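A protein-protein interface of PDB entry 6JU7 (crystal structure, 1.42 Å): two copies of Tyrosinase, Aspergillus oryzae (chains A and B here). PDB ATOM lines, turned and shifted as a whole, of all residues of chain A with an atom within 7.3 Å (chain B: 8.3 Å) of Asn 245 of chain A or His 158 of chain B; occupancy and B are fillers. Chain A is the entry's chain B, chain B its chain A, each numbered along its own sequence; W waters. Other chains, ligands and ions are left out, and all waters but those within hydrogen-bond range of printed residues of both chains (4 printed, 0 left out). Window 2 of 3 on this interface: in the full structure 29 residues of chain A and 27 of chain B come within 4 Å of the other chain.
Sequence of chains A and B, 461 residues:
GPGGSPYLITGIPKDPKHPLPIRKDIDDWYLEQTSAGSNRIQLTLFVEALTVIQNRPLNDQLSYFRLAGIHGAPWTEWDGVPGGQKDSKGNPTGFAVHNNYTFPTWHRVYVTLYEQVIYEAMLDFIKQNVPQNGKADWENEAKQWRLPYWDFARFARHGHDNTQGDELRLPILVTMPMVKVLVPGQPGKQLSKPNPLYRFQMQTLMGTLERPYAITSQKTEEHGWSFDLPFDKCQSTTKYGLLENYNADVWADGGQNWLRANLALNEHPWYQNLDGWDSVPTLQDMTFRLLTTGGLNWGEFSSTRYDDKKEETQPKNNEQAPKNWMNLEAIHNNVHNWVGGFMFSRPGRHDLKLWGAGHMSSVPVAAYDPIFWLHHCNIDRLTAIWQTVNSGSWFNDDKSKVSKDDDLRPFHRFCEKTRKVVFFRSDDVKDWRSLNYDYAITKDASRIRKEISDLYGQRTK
NE of Arg 169 of chain B sits at hydrogen-bond distance from OH of Tyr 246 of chain A (3.3 Å).
NH2 of Arg 169 of chain B is in hydrogen-bond range of O of Asn 245 of chain A (3.1 Å).
OE1 of Glu 167 of chain B sits at hydrogen-bond distance from OH of Tyr 246 of chain A, at 2.7 Å.
The guanidinium group of Arg 346 of chain A is in salt-bridge range of the side-chain carboxylate of Asp 166 of chain B (3.9 Å).
The side-chain carboxylate of Glu 167 of chain B lies within salt-bridge range of the guanidinium group of Arg 169 of chain B (2.9 Å).
NE1 of Trp 355 of chain A is in hydrogen-bond range of O of Ser 345 of chain A, 3.4 Å away.
A ring nitrogen (NE2) of His 158 of chain B is in hydrogen-bond range of the side-chain carboxylate (OD1) of Asp 166 of chain B (3.2 Å).
The backbone carbonyl oxygen (O) of Phe 344 of chain A sits at hydrogen-bond distance from the indole nitrogen (NE1) of Trp 355 of chain A (3.0 Å).
O of Glu 167 of chain B lies within hydrogen-bond range of N of Ala 156 of chain B (2.8 Å).
N of His 158 of chain B sits at hydrogen-bond distance from O of Thr 163 of chain B.
Among the printed residues, merely in contact across the chains: Asn 245 of chain A with His 158 of chain B, Asn 247 of chain A with Leu 31 of chain B, Arg 346 of chain A with Glu 167 of chain B and Trp 355 of chain A with Glu 167 of chain B.
Asn 245 of chain A touches two residues of chain B.
Printed residues of chain B within 4 Å of Tyr 246 of chain A: Glu 167 (2.7 Å) and Arg 169 (3.3 Å).
Of the printed residues of chain B, Asn 247 of chain A touches Leu 31 (3.5 Å).
His 158 of chain B touches one residue of chain A.
Of the printed residues of chain A, Asp 166 of chain B touches Arg 346 (3.8 Å).
Printed residues of chain A within 4 Å of Glu 167 of chain B: Tyr 246 (2.7 Å), Arg 346 (3.6 Å) and Trp 355 (3.5 Å).
Leu 168 of chain B touches none of the printed residues of chain A.
Printed residues of chain A within 4 Å of Arg 169 of chain B: Asn 245 and Tyr 246.
The nearest residue of chain A that does not touch His 158 of chain B is Glu 244 of chain A (6.0 Å).
The nearest printed residue of chain B that does not touch Trp 355 of chain A is Arg 169 of chain B (5.2 Å).
Hydrophobic or aromatic side chains of chain A within 4 Å of the printed part of chain B: Tyr 246 and Trp 355.
Of the 14 printed residues of chain B, 5 touch a printed residue of chain A.
Printed residues of chain B that touch a printed residue of chain A: Leu 31, His 158, Asp 166, Glu 167 and Arg 169.
Hydrophobic or aromatic side chains of chain B within 4 Å of the printed part of chain A: Leu 31 and His 158.
Among the printed residues, 8 pairs touch across the chains.
Among the printed residues, Asp or Glu carboxylates within 4 Å of a Lys or Arg side-chain nitrogen of the other chain: Arg 346 of chain A with Asp 166 of chain B.
No position is printed for both chains.
Water W4 bridges the side-chain carboxylate of Glu 167 of chain B (2.8 Å) and the side-chain hydroxyl of Tyr 246 of chain A (2.8 Å).
Water W1 bridges the guanidinium group of Arg 346 of chain A (2.8 Å) and the side-chain carboxylate of Glu 167 of chain B (3.1 Å).
Water W3 lies within hydrogen-bond range of the backbone NH of Gly 159 of chain B (2.9 Å), the backbone carbonyl oxygen of Asn 245 of chain A (3.1 Å) and the backbone NH of Asn 247 of chain A (3.5 Å).
Water W2 lies within hydrogen-bond range of the backbone NH (N) of Asn 247 of chain A (2.9 Å) and the guanidinium group (NH1) of Arg 169 of chain B (3.1 Å).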
ATOM      1  N   LEU A 243       0.643 -14.780  21.644  1.00  0.00           N
ATOM      2  CA  LEU A 243       1.178 -13.454  21.931  1.00  0.00           C
ATOM      3  C   LEU A 243       0.236 -12.750  22.902  1.00  0.00           C
ATOM      4  O   LEU A 243      -0.987 -12.888  22.725  1.00  0.00           O
ATOM      5  CB  LEU A 243       1.287 -12.588  20.670  1.00  0.00           C
ATOM      6  CG  LEU A 243       2.456 -12.854  19.720  1.00  0.00           C
ATOM      7  CD1 LEU A 243       2.399 -14.239  19.090  1.00  0.00           C
ATOM      8  CD2 LEU A 243       2.473 -11.773  18.639  1.00  0.00           C
ATOM      9  N   GLU A 244       0.797 -12.040  23.884  1.00  0.00           N
ATOM     10  CA  GLU A 244      -0.077 -11.288  24.797  1.00  0.00           C
ATOM     11  C   GLU A 244      -0.843 -10.196  24.059  1.00  0.00           C
ATOM     12  O   GLU A 244      -0.355  -9.624  23.089  1.00  0.00           O
ATOM     13  CB  GLU A 244       0.789 -10.667  25.908  1.00  0.00           C
ATOM     14  CG  GLU A 244      -0.030 -10.039  27.024  1.00  0.00           C
ATOM     15  CD  GLU A 244       0.788  -9.437  28.137  1.00  0.00           C
ATOM     16  OE1 GLU A 244       0.305  -9.419  29.293  1.00  0.00           O
ATOM     17  OE2 GLU A 244       1.905  -8.944  27.889  1.00  0.00           O
ATOM     18  N   ASN A 245      -2.057  -9.911  24.519  1.00  0.00           N
ATOM     19  CA  ASN A 245      -2.968  -8.902  24.002  1.00  0.00           C
ATOM     20  C   ASN A 245      -3.474  -9.213  22.596  1.00  0.00           C
ATOM     21  O   ASN A 245      -3.879  -8.318  21.845  1.00  0.00           O
ATOM     22  CB  ASN A 245      -2.345  -7.500  24.053  1.00  0.00           C
ATOM     23  CG  ASN A 245      -2.047  -7.114  25.498  1.00  0.00           C
ATOM     24  OD1 ASN A 245      -2.873  -7.252  26.388  1.00  0.00           O
ATOM     25  ND2 ASN A 245      -0.820  -6.667  25.723  1.00  0.00           N
ATOM     26  N   TYR A 246      -3.494 -10.491  22.249  1.00  0.00           N
ATOM     27  CA  TYR A 246      -4.206 -11.008  21.089  1.00  0.00           C
ATOM     28  C   TYR A 246      -5.472 -11.742  21.525  1.00  0.00           C
ATOM     29  O   TYR A 246      -5.522 -12.431  22.546  1.00  0.00           O
ATOM     30  CB  TYR A 246      -3.302 -11.964  20.276  1.00  0.00           C
ATOM     31  CG  TYR A 246      -2.328 -11.210  19.392  1.00  0.00           C
ATOM     32  CD1 TYR A 246      -2.423 -11.252  18.009  1.00  0.00           C
ATOM     33  CD2 TYR A 246      -1.314 -10.416  19.933  1.00  0.00           C
ATOM     34  CE1 TYR A 246      -1.547 -10.561  17.210  1.00  0.00           C
ATOM     35  CE2 TYR A 246      -0.428  -9.706  19.125  1.00  0.00           C
ATOM     36  CZ  TYR A 246      -0.546  -9.782  17.760  1.00  0.00           C
ATOM     37  OH  TYR A 246       0.295  -9.105  16.901  1.00  0.00           O
ATOM     38  N   ASN A 247      -6.515 -11.582  20.702  1.00  0.00           N
ATOM     39  CA  ASN A 247      -7.806 -12.222  20.944  1.00  0.00           C
ATOM     40  C   ASN A 247      -7.613 -13.719  21.125  1.00  0.00           C
ATOM     41  O   ASN A 247      -6.862 -14.344  20.373  1.00  0.00           O
ATOM     42  CB  ASN A 247      -8.709 -11.933  19.740  1.00  0.00           C
ATOM     43  CG  ASN A 247     -10.132 -12.425  19.899  1.00  0.00           C
ATOM     44  OD1 ASN A 247     -10.392 -13.630  19.906  1.00  0.00           O
ATOM     45  ND2 ASN A 247     -11.067 -11.476  20.015  1.00  0.00           N
ATOM     46  N   ALA A 248      -8.262 -14.290  22.135  1.00  0.00           N
ATOM     47  CA  ALA A 248      -8.061 -15.701  22.463  1.00  0.00           C
ATOM     48  C   ALA A 248      -8.517 -16.617  21.336  1.00  0.00           C
ATOM     49  O   ALA A 248      -8.126 -17.794  21.347  1.00  0.00           O
ATOM     50  CB  ALA A 248      -8.757 -16.064  23.771  1.00  0.00           C
ATOM     51  N   TRP A 251      -5.455 -17.732  19.687  1.00  0.00           N
ATOM     52  CA  TRP A 251      -4.768 -18.729  20.514  1.00  0.00           C
ATOM     53  C   TRP A 251      -5.297 -20.136  20.307  1.00  0.00           C
ATOM     54  O   TRP A 251      -4.539 -21.101  20.487  1.00  0.00           O
ATOM     55  CB  TRP A 251      -4.874 -18.376  21.994  1.00  0.00           C
ATOM     56  CG  TRP A 251      -4.196 -17.102  22.391  1.00  0.00           C
ATOM     57  CD1 TRP A 251      -3.305 -16.329  21.692  1.00  0.00           C
ATOM     58  CD2 TRP A 251      -4.399 -16.455  23.657  1.00  0.00           C
ATOM     59  NE1 TRP A 251      -2.938 -15.252  22.453  1.00  0.00           N
ATOM     60  CE2 TRP A 251      -3.599 -15.303  23.659  1.00  0.00           C
ATOM     61  CE3 TRP A 251      -5.194 -16.778  24.772  1.00  0.00           C
ATOM     62  CZ2 TRP A 251      -3.567 -14.447  24.757  1.00  0.00           C
ATOM     63  CZ3 TRP A 251      -5.162 -15.919  25.862  1.00  0.00           C
ATOM     64  CH2 TRP A 251      -4.353 -14.773  25.836  1.00  0.00           C
ATOM     65  N   PHE A 344       6.125 -14.604  25.179  1.00  0.00           N
ATOM     66  CA  PHE A 344       4.684 -14.362  25.122  1.00  0.00           C
ATOM     67  C   PHE A 344       4.424 -12.867  25.145  1.00  0.00           C
ATOM     68  O   PHE A 344       3.674 -12.301  24.341  1.00  0.00           O
ATOM     69  CB  PHE A 344       4.017 -15.085  26.306  1.00  0.00           C
ATOM     70  CG  PHE A 344       2.532 -14.867  26.443  1.00  0.00           C
ATOM     71  CD1 PHE A 344       1.674 -15.317  25.447  1.00  0.00           C
ATOM     72  CD2 PHE A 344       1.987 -14.203  27.536  1.00  0.00           C
ATOM     73  CE1 PHE A 344       0.311 -15.113  25.568  1.00  0.00           C
ATOM     74  CE2 PHE A 344       0.630 -14.010  27.669  1.00  0.00           C
ATOM     75  CZ  PHE A 344      -0.201 -14.458  26.661  1.00  0.00           C
ATOM     76  N   SER A 345       4.997 -12.166  26.131  1.00  0.00           N
ATOM     77  CA  SER A 345       4.816 -10.713  26.186  1.00  0.00           C
ATOM     78  C   SER A 345       5.672  -9.989  25.151  1.00  0.00           C
ATOM     79  O   SER A 345       6.718 -10.495  24.702  1.00  0.00           O
ATOM     80  CB  SER A 345       5.069 -10.201  27.605  1.00  0.00           C
ATOM     81  OG  SER A 345       6.436 -10.378  27.958  1.00  0.00           O
ATOM     82  N   ARG A 346       5.196  -8.825  24.699  1.00  0.00           N
ATOM     83  CA  ARG A 346       5.869  -8.091  23.629  1.00  0.00           C
ATOM     84  C   ARG A 346       7.238  -7.626  24.113  1.00  0.00           C
ATOM     85  O   ARG A 346       7.303  -6.969  25.145  1.00  0.00           O
ATOM     86  CB  ARG A 346       5.042  -6.880  23.155  1.00  0.00           C
ATOM     87  CG  ARG A 346       5.454  -6.370  21.783  1.00  0.00           C
ATOM     88  CD  ARG A 346       4.540  -5.325  21.159  1.00  0.00           C
ATOM     89  NE  ARG A 346       4.699  -5.180  19.711  1.00  0.00           N
ATOM     90  CZ  ARG A 346       5.003  -4.116  18.996  1.00  0.00           C
ATOM     91  NH1 ARG A 346       5.117  -4.163  17.663  1.00  0.00           N
ATOM     92  NH2 ARG A 346       5.214  -2.939  19.585  1.00  0.00           N
ATOM     93  N   TRP A 355       9.230 -12.524  18.406  1.00  0.00           N
ATOM     94  CA  TRP A 355       8.112 -12.524  19.344  1.00  0.00           C
ATOM     95  C   TRP A 355       7.165 -13.698  19.116  1.00  0.00           C
ATOM     96  O   TRP A 355       6.794 -14.003  17.979  1.00  0.00           O
ATOM     97  CB  TRP A 355       7.358 -11.206  19.226  1.00  0.00           C
ATOM     98  CG  TRP A 355       6.251 -10.964  20.198  1.00  0.00           C
ATOM     99  CD1 TRP A 355       5.993 -11.543  21.408  1.00  0.00           C
ATOM    100  CD2 TRP A 355       5.209  -9.996  19.968  1.00  0.00           C
ATOM    101  NE1 TRP A 355       4.847 -10.990  21.943  1.00  0.00           N
ATOM    102  CE2 TRP A 355       4.358 -10.047  21.079  1.00  0.00           C
ATOM    103  CE3 TRP A 355       4.939  -9.106  18.922  1.00  0.00           C
ATOM    104  CZ2 TRP A 355       3.224  -9.232  21.203  1.00  0.00           C
ATOM    105  CZ3 TRP A 355       3.817  -8.299  19.042  1.00  0.00           C
ATOM    106  CH2 TRP A 355       2.974  -8.371  20.170  1.00  0.00           C
ATOM    107  N   LEU B  31     -15.314  -8.262  16.825  1.00  0.00           N
ATOM    108  CA  LEU B  31     -15.650  -8.157  18.245  1.00  0.00           C
ATOM    109  C   LEU B  31     -17.129  -7.884  18.468  1.00  0.00           C
ATOM    110  O   LEU B  31     -17.712  -8.388  19.435  1.00  0.00           O
ATOM    111  CB  LEU B  31     -14.853  -7.015  18.873  1.00  0.00           C
ATOM    112  CG  LEU B  31     -13.346  -7.234  18.968  1.00  0.00           C
ATOM    113  CD1 LEU B  31     -12.716  -6.071  19.718  1.00  0.00           C
ATOM    114  CD2 LEU B  31     -12.982  -8.546  19.641  1.00  0.00           C
ATOM    115  N   PHE B 155      -3.859   1.249  15.053  1.00  0.00           N
ATOM    116  CA  PHE B 155      -3.295   0.262  15.975  1.00  0.00           C
ATOM    117  C   PHE B 155      -4.375  -0.715  16.413  1.00  0.00           C
ATOM    118  O   PHE B 155      -5.492  -0.292  16.756  1.00  0.00           O
ATOM    119  CB  PHE B 155      -2.704   0.980  17.188  1.00  0.00           C
ATOM    120  CG  PHE B 155      -1.527   1.868  16.859  1.00  0.00           C
ATOM    121  CD1 PHE B 155      -0.502   1.445  16.021  1.00  0.00           C
ATOM    122  CD2 PHE B 155      -1.432   3.141  17.399  1.00  0.00           C
ATOM    123  CE1 PHE B 155       0.596   2.250  15.775  1.00  0.00           C
ATOM    124  CE2 PHE B 155      -0.329   3.955  17.170  1.00  0.00           C
ATOM    125  CZ  PHE B 155       0.699   3.506  16.354  1.00  0.00           C
ATOM    126  N   ALA B 156      -4.034  -2.007  16.402  1.00  0.00           N
ATOM    127  CA  ALA B 156      -4.983  -3.003  16.890  1.00  0.00           C
ATOM    128  C   ALA B 156      -5.336  -2.762  18.359  1.00  0.00           C
ATOM    129  O   ALA B 156      -4.453  -2.401  19.141  1.00  0.00           O
ATOM    130  CB  ALA B 156      -4.441  -4.424  16.765  1.00  0.00           C
ATOM    131  N   ARG B 157      -6.586  -2.967  18.739  1.00  0.00           N
ATOM    132  CA  ARG B 157      -7.004  -2.794  20.126  1.00  0.00           C
ATOM    133  C   ARG B 157      -6.505  -3.948  20.986  1.00  0.00           C
ATOM    134  O   ARG B 157      -6.246  -5.050  20.499  1.00  0.00           O
ATOM    135  CB  ARG B 157      -8.534  -2.715  20.187  1.00  0.00           C
ATOM    136  CG  ARG B 157      -9.056  -1.301  19.976  1.00  0.00           C
ATOM    137  CD  ARG B 157      -8.708  -0.781  18.586  1.00  0.00           C
ATOM    138  NE  ARG B 157      -9.563  -1.370  17.566  1.00  0.00           N
ATOM    139  CZ  ARG B 157      -9.264  -1.586  16.289  1.00  0.00           C
ATOM    140  NH1 ARG B 157      -8.074  -1.270  15.789  1.00  0.00           N
ATOM    141  NH2 ARG B 157     -10.160  -2.132  15.475  1.00  0.00           N
ATOM    142  N   HIS B 158      -6.384  -3.682  22.276  1.00  0.00           N
ATOM    143  CA  HIS B 158      -5.982  -4.707  23.232  1.00  0.00           C
ATOM    144  C   HIS B 158      -7.199  -5.092  24.064  1.00  0.00           C
ATOM    145  O   HIS B 158      -7.535  -4.372  25.007  1.00  0.00           O
ATOM    146  CB  HIS B 158      -4.871  -4.219  24.165  1.00  0.00           C
ATOM    147  CG  HIS B 158      -3.560  -4.016  23.468  1.00  0.00           C
ATOM    148  ND1 HIS B 158      -2.420  -3.581  24.099  1.00  0.00           N
ATOM    149  CD2 HIS B 158      -3.205  -4.205  22.175  1.00  0.00           C
ATOM    150  CE1 HIS B 158      -1.423  -3.502  23.240  1.00  0.00           C
ATOM    151  NE2 HIS B 158      -1.878  -3.867  22.055  1.00  0.00           N
ATOM    152  N   GLY B 159      -7.804  -6.212  23.700  1.00  0.00           N
ATOM    153  CA  GLY B 159      -9.080  -6.584  24.291  1.00  0.00           C
ATOM    154  C   GLY B 159     -10.208  -5.748  23.700  1.00  0.00           C
ATOM    155  O   GLY B 159     -10.231  -5.564  22.476  1.00  0.00           O
ATOM    156  N   THR B 163      -9.079  -0.693  25.097  1.00  0.00           N
ATOM    157  CA  THR B 163      -7.713  -0.216  25.314  1.00  0.00           C
ATOM    158  C   THR B 163      -6.983   0.007  23.991  1.00  0.00           C
ATOM    159  O   THR B 163      -7.069  -0.847  23.105  1.00  0.00           O
ATOM    160  CB  THR B 163      -6.905  -1.205  26.178  1.00  0.00           C
ATOM    161  N   GLN B 164      -6.277   1.122  23.889  1.00  0.00           N
ATOM    162  CA  GLN B 164      -5.491   1.509  22.728  1.00  0.00           C
ATOM    163  C   GLN B 164      -4.217   0.675  22.612  1.00  0.00           C
ATOM    164  O   GLN B 164      -3.471   0.510  23.585  1.00  0.00           O
ATOM    165  N   GLY B 165      -3.971   0.144  21.420  1.00  0.00           N
ATOM    166  CA  GLY B 165      -2.816  -0.700  21.155  1.00  0.00           C
ATOM    167  C   GLY B 165      -1.618   0.096  20.670  1.00  0.00           C
ATOM    168  O   GLY B 165      -1.651   1.326  20.641  1.00  0.00           O
ATOM    169  N   ASP B 166      -0.575  -0.606  20.249  1.00  0.00           N
ATOM    170  CA  ASP B 166       0.723  -0.072  19.901  1.00  0.00           C
ATOM    171  C   ASP B 166       1.260  -0.566  18.563  1.00  0.00           C
ATOM    172  O   ASP B 166       2.327  -0.157  18.101  1.00  0.00           O
ATOM    173  CB  ASP B 166       1.717  -0.451  21.004  1.00  0.00           C
ATOM    174  CG  ASP B 166       1.726  -1.900  21.427  1.00  0.00           C
ATOM    175  OD1 ASP B 166       0.959  -2.750  20.934  1.00  0.00           O
ATOM    176  OD2 ASP B 166       2.552  -2.238  22.311  1.00  0.00           O
ATOM    177  N   GLU B 167       0.518  -1.469  17.955  1.00  0.00           N
ATOM    178  CA  GLU B 167       0.972  -2.330  16.880  1.00  0.00           C
ATOM    179  C   GLU B 167      -0.090  -2.356  15.786  1.00  0.00           C
ATOM    180  O   GLU B 167      -1.280  -2.547  16.059  1.00  0.00           O
ATOM    181  CB  GLU B 167       1.224  -3.758  17.414  1.00  0.00           C
ATOM    182  CG  GLU B 167       1.759  -4.734  16.367  1.00  0.00           C
ATOM    183  CD  GLU B 167       1.745  -6.193  16.750  1.00  0.00           C
ATOM    184  OE1 GLU B 167       1.028  -6.596  17.710  1.00  0.00           O
ATOM    185  OE2 GLU B 167       2.433  -7.018  16.077  1.00  0.00           O
ATOM    186  N   LEU B 168       0.335  -2.189  14.548  1.00  0.00           N
ATOM    187  CA  LEU B 168      -0.515  -2.491  13.404  1.00  0.00           C
ATOM    188  C   LEU B 168      -0.538  -3.994  13.194  1.00  0.00           C
ATOM    189  O   LEU B 168       0.470  -4.671  13.449  1.00  0.00           O
ATOM    190  CB  LEU B 168       0.049  -1.817  12.150  1.00  0.00           C
ATOM    191  CG  LEU B 168       0.242  -0.301  12.256  1.00  0.00           C
ATOM    192  CD1 LEU B 168       0.918   0.202  10.991  1.00  0.00           C
ATOM    193  CD2 LEU B 168      -1.104   0.380  12.493  1.00  0.00           C
ATOM    194  N   ARG B 169      -1.671  -4.538  12.786  1.00  0.00           N
ATOM    195  CA  ARG B 169      -1.785  -5.989  12.681  1.00  0.00           C
ATOM    196  C   ARG B 169      -2.707  -6.382  11.533  1.00  0.00           C
ATOM    197  O   ARG B 169      -3.683  -5.657  11.253  1.00  0.00           O
ATOM    198  CB  ARG B 169      -2.431  -6.564  13.948  1.00  0.00           C
ATOM    199  CG  ARG B 169      -1.665  -6.390  15.245  1.00  0.00           C
ATOM    200  CD  ARG B 169      -2.409  -7.142  16.356  1.00  0.00           C
ATOM    201  NE  ARG B 169      -1.910  -6.764  17.676  1.00  0.00           N
ATOM    202  CZ  ARG B 169      -2.521  -7.102  18.800  1.00  0.00           C
ATOM    203  NH1 ARG B 169      -3.653  -7.812  18.745  1.00  0.00           N
ATOM    204  NH2 ARG B 169      -1.991  -6.722  19.960  1.00  0.00           N
ATOM    205  N   ILE B 172      -7.790  -9.841  13.028  1.00  0.00           N
ATOM    206  CA  ILE B 172      -7.969 -11.015  13.881  1.00  0.00           C
ATOM    207  C   ILE B 172      -8.467 -12.206  13.067  1.00  0.00           C
ATOM    208  O   ILE B 172      -7.885 -13.290  13.103  1.00  0.00           O
ATOM    209  CB  ILE B 172      -8.965 -10.726  15.023  1.00  0.00           C
ATOM    210  CG1 ILE B 172      -8.490  -9.624  15.974  1.00  0.00           C
ATOM    211  CG2 ILE B 172      -9.325 -12.003  15.755  1.00  0.00           C
ATOM    212  CD1 ILE B 172      -9.631  -8.955  16.732  1.00  0.00           C
HETATM  213  O   HOH W   1       5.415  -6.230  15.771  1.00  0.00           O
HETATM  214  O   HOH W   2      -6.271  -9.399  18.800  1.00  0.00           O
HETATM  215  O   HOH W   3      -6.966  -8.385  22.019  1.00  0.00           O
HETATM  216  O   HOH W   4       2.750  -9.781  15.647  1.00  0.00           O
